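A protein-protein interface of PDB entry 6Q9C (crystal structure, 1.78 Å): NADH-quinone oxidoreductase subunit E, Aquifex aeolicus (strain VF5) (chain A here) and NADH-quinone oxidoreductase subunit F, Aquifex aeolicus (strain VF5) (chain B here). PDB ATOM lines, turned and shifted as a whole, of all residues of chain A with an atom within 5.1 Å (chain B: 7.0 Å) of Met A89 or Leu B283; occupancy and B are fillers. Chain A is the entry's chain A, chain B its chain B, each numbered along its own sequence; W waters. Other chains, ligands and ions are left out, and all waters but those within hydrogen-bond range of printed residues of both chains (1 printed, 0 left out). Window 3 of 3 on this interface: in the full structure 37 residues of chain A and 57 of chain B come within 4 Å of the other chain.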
ATOM      1  N   VAL A  85      36.166  -6.328  15.002  1.00  0.00           N
ATOM      2  CA  VAL A  85      35.248  -7.194  15.806  1.00  0.00           C
ATOM      3  C   VAL A  85      35.870  -7.441  17.185  1.00  0.00           C
ATOM      4  O   VAL A  85      35.171  -7.244  18.190  1.00  0.00           O
ATOM      5  CB  VAL A  85      34.870  -8.505  15.096  1.00  0.00           C
ATOM      6  CG1 VAL A  85      33.782  -9.243  15.863  1.00  0.00           C
ATOM      7  CG2 VAL A  85      34.433  -8.258  13.656  1.00  0.00           C
ATOM      8  N   CYS A  86      37.140  -7.824  17.259  1.00  0.00           N
ATOM      9  CA  CYS A  86      37.818  -8.019  18.563  1.00  0.00           C
ATOM     10  C   CYS A  86      37.799  -6.698  19.349  1.00  0.00           C
ATOM     11  O   CYS A  86      37.557  -6.745  20.572  1.00  0.00           O
ATOM     12  CB  CYS A  86      39.201  -8.618  18.362  1.00  0.00           C
ATOM     13  SG  CYS A  86      39.084 -10.306  17.715  1.00  0.00           S
ATOM     14  N   HIS A  87      37.959  -5.551  18.684  1.00  0.00           N
ATOM     15  CA  HIS A  87      37.902  -4.235  19.375  1.00  0.00           C
ATOM     16  C   HIS A  87      36.517  -4.049  20.017  1.00  0.00           C
ATOM     17  O   HIS A  87      36.469  -3.715  21.214  1.00  0.00           O
ATOM     18  CB  HIS A  87      38.279  -3.079  18.446  1.00  0.00           C
ATOM     19  CG  HIS A  87      38.231  -1.770  19.159  1.00  0.00           C
ATOM     20  ND1 HIS A  87      39.246  -1.352  19.998  1.00  0.00           N
ATOM     21  CD2 HIS A  87      37.264  -0.833  19.226  1.00  0.00           C
ATOM     22  CE1 HIS A  87      38.927  -0.187  20.515  1.00  0.00           C
ATOM     23  NE2 HIS A  87      37.713   0.155  20.057  1.00  0.00           N
ATOM     24  N   LEU A  88      35.441  -4.290  19.263  1.00  0.00           N
ATOM     25  CA  LEU A  88      34.031  -4.191  19.738  1.00  0.00           C
ATOM     26  C   LEU A  88      33.800  -5.109  20.945  1.00  0.00           C
ATOM     27  O   LEU A  88      33.050  -4.700  21.839  1.00  0.00           O
ATOM     28  CB  LEU A  88      33.068  -4.570  18.610  1.00  0.00           C
ATOM     29  CG  LEU A  88      32.764  -3.478  17.587  1.00  0.00           C
ATOM     30  CD1 LEU A  88      32.018  -4.070  16.401  1.00  0.00           C
ATOM     31  CD2 LEU A  88      31.957  -2.346  18.212  1.00  0.00           C
ATOM     32  N   MET A  89      34.395  -6.307  20.952  1.00  0.00           N
ATOM     33  CA  MET A  89      34.028  -7.403  21.889  1.00  0.00           C
ATOM     34  C   MET A  89      35.032  -7.530  23.045  1.00  0.00           C
ATOM     35  O   MET A  89      34.752  -8.345  23.943  1.00  0.00           O
ATOM     36  CB  MET A  89      33.928  -8.737  21.141  1.00  0.00           C
ATOM     37  CG  MET A  89      32.949  -8.716  19.980  1.00  0.00           C
ATOM     38  SD  MET A  89      31.306  -8.080  20.399  1.00  0.00           S
ATOM     39  CE  MET A  89      30.706  -9.383  21.474  1.00  0.00           C
ATOM     40  N   GLY A  90      36.147  -6.785  23.044  1.00  0.00           N
ATOM     41  CA  GLY A  90      36.983  -6.615  24.255  1.00  0.00           C
ATOM     42  C   GLY A  90      38.484  -6.821  24.067  1.00  0.00           C
ATOM     43  O   GLY A  90      39.125  -7.298  25.024  1.00  0.00           O
ATOM     44  N   THR A  91      39.076  -6.405  22.944  1.00  0.00           N
ATOM     45  CA  THR A  91      40.557  -6.396  22.767  1.00  0.00           C
ATOM     46  C   THR A  91      41.222  -5.732  23.982  1.00  0.00           C
ATOM     47  O   THR A  91      42.235  -6.269  24.460  1.00  0.00           O
ATOM     48  CB  THR A  91      40.984  -5.676  21.481  1.00  0.00           C
ATOM     49  OG1 THR A  91      40.511  -6.444  20.378  1.00  0.00           O
ATOM     50  CG2 THR A  91      42.481  -5.493  21.361  1.00  0.00           C
ATOM     51  N   ALA A 129      35.593 -13.599  19.203  1.00  0.00           N
ATOM     52  CA  ALA A 129      36.276 -12.364  19.652  1.00  0.00           C
ATOM     53  C   ALA A 129      36.112 -12.189  21.161  1.00  0.00           C
ATOM     54  O   ALA A 129      35.097 -12.611  21.727  1.00  0.00           O
ATOM     55  CB  ALA A 129      35.704 -11.184  18.906  1.00  0.00           C
ATOM     56  N   PRO A 130      37.087 -11.581  21.878  1.00  0.00           N
ATOM     57  CA  PRO A 130      38.380 -11.188  21.319  1.00  0.00           C
ATOM     58  C   PRO A 130      39.340 -12.380  21.184  1.00  0.00           C
ATOM     59  O   PRO A 130      39.398 -13.194  22.079  1.00  0.00           O
ATOM     60  CB  PRO A 130      38.926 -10.146  22.307  1.00  0.00           C
ATOM     61  CG  PRO A 130      38.244 -10.454  23.615  1.00  0.00           C
ATOM     62  CD  PRO A 130      36.960 -11.196  23.290  1.00  0.00           C
ATOM     63  N   SER B 254      29.205 -12.054  13.113  1.00  0.00           N
ATOM     64  CA  SER B 254      29.964 -11.682  14.336  1.00  0.00           C
ATOM     65  C   SER B 254      29.471 -10.349  14.922  1.00  0.00           C
ATOM     66  O   SER B 254      28.547  -9.719  14.348  1.00  0.00           O
ATOM     67  CB  SER B 254      31.447 -11.656  14.044  1.00  0.00           C
ATOM     68  OG  SER B 254      31.763 -10.656  13.093  1.00  0.00           O
ATOM     69  N   GLY B 255      30.085  -9.933  16.031  1.00  0.00           N
ATOM     70  CA  GLY B 255      29.710  -8.719  16.775  1.00  0.00           C
ATOM     71  C   GLY B 255      28.552  -8.992  17.716  1.00  0.00           C
ATOM     72  O   GLY B 255      28.561 -10.046  18.380  1.00  0.00           O
ATOM     73  N   LYS B 256      27.566  -8.095  17.739  1.00  0.00           N
ATOM     74  CA  LYS B 256      26.543  -8.010  18.812  1.00  0.00           C
ATOM     75  C   LYS B 256      25.340  -8.892  18.469  1.00  0.00           C
ATOM     76  O   LYS B 256      24.212  -8.386  18.526  1.00  0.00           O
ATOM     77  CB  LYS B 256      26.136  -6.550  19.018  1.00  0.00           C
ATOM     78  CG  LYS B 256      27.280  -5.616  19.375  1.00  0.00           C
ATOM     79  CD  LYS B 256      28.074  -6.052  20.591  1.00  0.00           C
ATOM     80  CE  LYS B 256      29.186  -5.084  20.939  1.00  0.00           C
ATOM     81  NZ  LYS B 256      28.663  -3.739  21.280  1.00  0.00           N
ATOM     82  N   VAL B 257      25.574 -10.171  18.162  1.00  0.00           N
ATOM     83  CA  VAL B 257      24.494 -11.186  17.978  1.00  0.00           C
ATOM     84  C   VAL B 257      24.630 -12.231  19.091  1.00  0.00           C
ATOM     85  O   VAL B 257      25.738 -12.380  19.636  1.00  0.00           O
ATOM     86  CB  VAL B 257      24.529 -11.836  16.580  1.00  0.00           C
ATOM     87  CG1 VAL B 257      24.268 -10.819  15.481  1.00  0.00           C
ATOM     88  CG2 VAL B 257      25.828 -12.586  16.329  1.00  0.00           C
ATOM     89  N   LYS B 258      23.543 -12.935  19.403  1.00  0.00           N
ATOM     90  CA  LYS B 258      23.513 -13.963  20.473  1.00  0.00           C
ATOM     91  C   LYS B 258      24.247 -15.224  20.006  1.00  0.00           C
ATOM     92  O   LYS B 258      24.864 -15.873  20.862  1.00  0.00           O
ATOM     93  CB  LYS B 258      22.072 -14.275  20.881  1.00  0.00           C
ATOM     94  CG  LYS B 258      21.333 -13.129  21.556  1.00  0.00           C
ATOM     95  CD  LYS B 258      20.083 -13.574  22.293  1.00  0.00           C
ATOM     96  CE  LYS B 258      19.164 -12.436  22.686  1.00  0.00           C
ATOM     97  NZ  LYS B 258      18.585 -11.764  21.497  1.00  0.00           N
ATOM     98  N   LYS B 259      24.184 -15.566  18.713  1.00  0.00           N
ATOM     99  CA  LYS B 259      24.773 -16.823  18.166  1.00  0.00           C
ATOM    100  C   LYS B 259      25.754 -16.511  17.043  1.00  0.00           C
ATOM    101  O   LYS B 259      25.536 -16.906  15.896  1.00  0.00           O
ATOM    102  CB  LYS B 259      23.681 -17.763  17.648  1.00  0.00           C
ATOM    103  CG  LYS B 259      22.700 -18.285  18.686  1.00  0.00           C
ATOM    104  CD  LYS B 259      21.480 -18.958  18.069  1.00  0.00           C
ATOM    105  CE  LYS B 259      21.809 -19.905  16.929  1.00  0.00           C
ATOM    106  NZ  LYS B 259      20.590 -20.400  16.245  1.00  0.00           N
ATOM    107  N   PRO B 260      26.898 -15.852  17.334  1.00  0.00           N
ATOM    108  CA  PRO B 260      27.880 -15.559  16.294  1.00  0.00           C
ATOM    109  C   PRO B 260      28.455 -16.888  15.783  1.00  0.00           C
ATOM    110  O   PRO B 260      28.618 -17.807  16.580  1.00  0.00           O
ATOM    111  CB  PRO B 260      28.916 -14.677  17.012  1.00  0.00           C
ATOM    112  CG  PRO B 260      28.821 -15.117  18.459  1.00  0.00           C
ATOM    113  CD  PRO B 260      27.357 -15.444  18.669  1.00  0.00           C
ATOM    114  N   GLY B 280      20.048 -15.441  16.191  1.00  0.00           N
ATOM    115  CA  GLY B 280      19.405 -15.364  17.518  1.00  0.00           C
ATOM    116  C   GLY B 280      19.085 -13.942  17.952  1.00  0.00           C
ATOM    117  O   GLY B 280      18.702 -13.759  19.124  1.00  0.00           O
ATOM    118  N   GLY B 281      19.194 -12.968  17.047  1.00  0.00           N
ATOM    119  CA  GLY B 281      18.950 -11.550  17.360  1.00  0.00           C
ATOM    120  C   GLY B 281      20.167 -10.917  18.005  1.00  0.00           C
ATOM    121  O   GLY B 281      21.247 -11.532  17.972  1.00  0.00           O
ATOM    122  N   THR B 282      20.010  -9.720  18.562  1.00  0.00           N
ATOM    123  CA  THR B 282      21.144  -8.897  19.060  1.00  0.00           C
ATOM    124  C   THR B 282      21.415  -9.225  20.531  1.00  0.00           C
ATOM    125  O   THR B 282      20.476  -9.668  21.215  1.00  0.00           O
ATOM    126  CB  THR B 282      20.854  -7.409  18.855  1.00  0.00           C
ATOM    127  OG1 THR B 282      19.651  -7.119  19.564  1.00  0.00           O
ATOM    128  CG2 THR B 282      20.721  -7.039  17.392  1.00  0.00           C
ATOM    129  N   LEU B 283      22.651  -9.001  20.996  1.00  0.00           N
ATOM    130  CA  LEU B 283      23.003  -9.066  22.443  1.00  0.00           C
ATOM    131  C   LEU B 283      22.175  -8.013  23.186  1.00  0.00           C
ATOM    132  O   LEU B 283      22.123  -6.858  22.715  1.00  0.00           O
ATOM    133  CB  LEU B 283      24.504  -8.824  22.638  1.00  0.00           C
ATOM    134  CG  LEU B 283      25.419  -9.991  22.268  1.00  0.00           C
ATOM    135  CD1 LEU B 283      26.880  -9.588  22.408  1.00  0.00           C
ATOM    136  CD2 LEU B 283      25.135 -11.224  23.114  1.00  0.00           C
ATOM    137  N   GLY B 284      21.523  -8.414  24.282  1.00  0.00           N
ATOM    138  CA  GLY B 284      20.680  -7.542  25.121  1.00  0.00           C
ATOM    139  C   GLY B 284      19.443  -7.053  24.382  1.00  0.00           C
ATOM    140  O   GLY B 284      18.791  -6.132  24.894  1.00  0.00           O
ATOM    141  N   ASN B 285      19.126  -7.642  23.219  1.00  0.00           N
ATOM    142  CA  ASN B 285      17.966  -7.255  22.368  1.00  0.00           C
ATOM    143  C   ASN B 285      18.043  -5.757  22.045  1.00  0.00           C
ATOM    144  O   ASN B 285      16.981  -5.116  21.906  1.00  0.00           O
ATOM    145  CB  ASN B 285      16.640  -7.633  23.032  1.00  0.00           C
ATOM    146  CG  ASN B 285      16.453  -9.131  23.131  1.00  0.00           C
ATOM    147  OD1 ASN B 285      16.846  -9.867  22.231  1.00  0.00           O
ATOM    148  ND2 ASN B 285      15.835  -9.592  24.204  1.00  0.00           N
ATOM    149  N   LYS B 286      19.259  -5.220  21.930  1.00  0.00           N
ATOM    150  CA  LYS B 286      19.499  -3.806  21.559  1.00  0.00           C
ATOM    151  C   LYS B 286      19.200  -3.659  20.064  1.00  0.00           C
ATOM    152  O   LYS B 286      19.288  -4.670  19.332  1.00  0.00           O
ATOM    153  CB  LYS B 286      20.921  -3.390  21.951  1.00  0.00           C
ATOM    154  CG  LYS B 286      21.167  -3.407  23.456  1.00  0.00           C
ATOM    155  CD  LYS B 286      22.491  -2.831  23.900  1.00  0.00           C
ATOM    156  CE  LYS B 286      22.610  -2.765  25.412  1.00  0.00           C
ATOM    157  NZ  LYS B 286      23.999  -2.465  25.835  1.00  0.00           N
ATOM    158  N   LYS B 287      18.835  -2.452  19.638  1.00  0.00           N
ATOM    159  CA  LYS B 287      18.506  -2.155  18.223  1.00  0.00           C
ATOM    160  C   LYS B 287      19.786  -2.260  17.383  1.00  0.00           C
ATOM    161  O   LYS B 287      20.868  -1.841  17.864  1.00  0.00           O
ATOM    162  CB  LYS B 287      17.834  -0.783  18.119  1.00  0.00           C
ATOM    163  CG  LYS B 287      16.394  -0.753  18.621  1.00  0.00           C
ATOM    164  CD  LYS B 287      15.848   0.631  18.910  1.00  0.00           C
ATOM    165  CE  LYS B 287      16.025   1.610  17.768  1.00  0.00           C
ATOM    166  NZ  LYS B 287      17.303   2.359  17.864  1.00  0.00           N
ATOM    167  N   VAL B 323      27.694  -7.119  13.174  1.00  0.00           N
ATOM    168  CA  VAL B 323      26.525  -6.380  13.729  1.00  0.00           C
ATOM    169  C   VAL B 323      27.014  -5.394  14.794  1.00  0.00           C
ATOM    170  O   VAL B 323      27.649  -5.831  15.769  1.00  0.00           O
ATOM    171  CB  VAL B 323      25.464  -7.346  14.283  1.00  0.00           C
ATOM    172  CG1 VAL B 323      24.234  -6.598  14.766  1.00  0.00           C
ATOM    173  CG2 VAL B 323      25.084  -8.392  13.248  1.00  0.00           C
ATOM    174  N   THR B 325      25.303  -2.437  17.395  1.00  0.00           N
ATOM    175  CA  THR B 325      24.015  -2.055  18.018  1.00  0.00           C
ATOM    176  C   THR B 325      24.076  -0.589  18.458  1.00  0.00           C
ATOM    177  O   THR B 325      25.142   0.049  18.293  1.00  0.00           O
ATOM    178  CB  THR B 325      23.644  -3.053  19.120  1.00  0.00           C
ATOM    179  OG1 THR B 325      24.733  -3.111  20.035  1.00  0.00           O
ATOM    180  CG2 THR B 325      23.357  -4.429  18.565  1.00  0.00           C
HETATM  181  O   HOH W   1      31.382  -2.795  22.435  1.00  0.00           O
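Val A85 touches Ser B254. CG1 of Val A85 touches N of Gly B255 (3.8 Å). Leu A88 touches Lys B256. O of Gly B255 touches CE of Met A89 (3.8 Å). Met A89 touches Lys B256 (SD to CE, 3.7 Å). Met A89 touches Leu B283 (CE to CD1, 3.9 Å).
Water W1 bridges O of Leu A88 and NZ of Lys B256.
The backbone carbonyl oxygen (O) of Lys B256 sits at hydrogen-bond distance from the backbone NH (N) of Leu B283. The backbone NH (N) of Lys B256 lies within hydrogen-bond range of the backbone carbonyl oxygen (O) of Val B323. The backbone NH of Val B323 is in hydrogen-bond range of the backbone carbonyl oxygen of Ser B254 (3.0 Å).
Of the printed residues of chain B, Val A85 touches Ser B254 and Gly B255. Of the printed residues of chain B, Leu A88 touches Lys B256. Met A89 touches just these residues of chain B: Gly B255, Lys B256 and Leu B283. Printed residues of chain A within 4 Å of Ser B254: Val A85 (3.6 Å). Of the printed residues of chain A, Lys B256 touches Leu A88 (3.99 Å) and Met A89 (3.7 Å). Of chain A, only Met A89 comes within 4 Å of Leu B283. The nearest printed residue of chain A that does not touch Leu B283 is Leu A88 (7.9 Å).
Of the 9 printed residues of chain A, 3 touch a printed residue of chain B. Printed residues of chain A that touch a printed residue of chain B: Val A85, Leu A88 and Met A89. Hydrophobic or aromatic side chains of chain A that line the printed part of chain B: Val A85 and Met A89. Along chain A the printed residues that touch a printed residue of chain B span positions 85 to 89. Printed residues of chain B that touch a printed residue of chain A: Ser B254, Gly B255, Lys B256 and Leu B283. Hydrophobic or aromatic side chains of chain B within 4 Å of the printed part of chain A: Leu B283. Along chain B the printed residues that touch a printed residue of chain A span positions 254 to 283. Among the printed residues, 6 pairs touch across the chains. Among the printed residues, no Asp or Glu carboxylate lies within 4 Å of a Lys or Arg side-chain nitrogen of the other chain.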
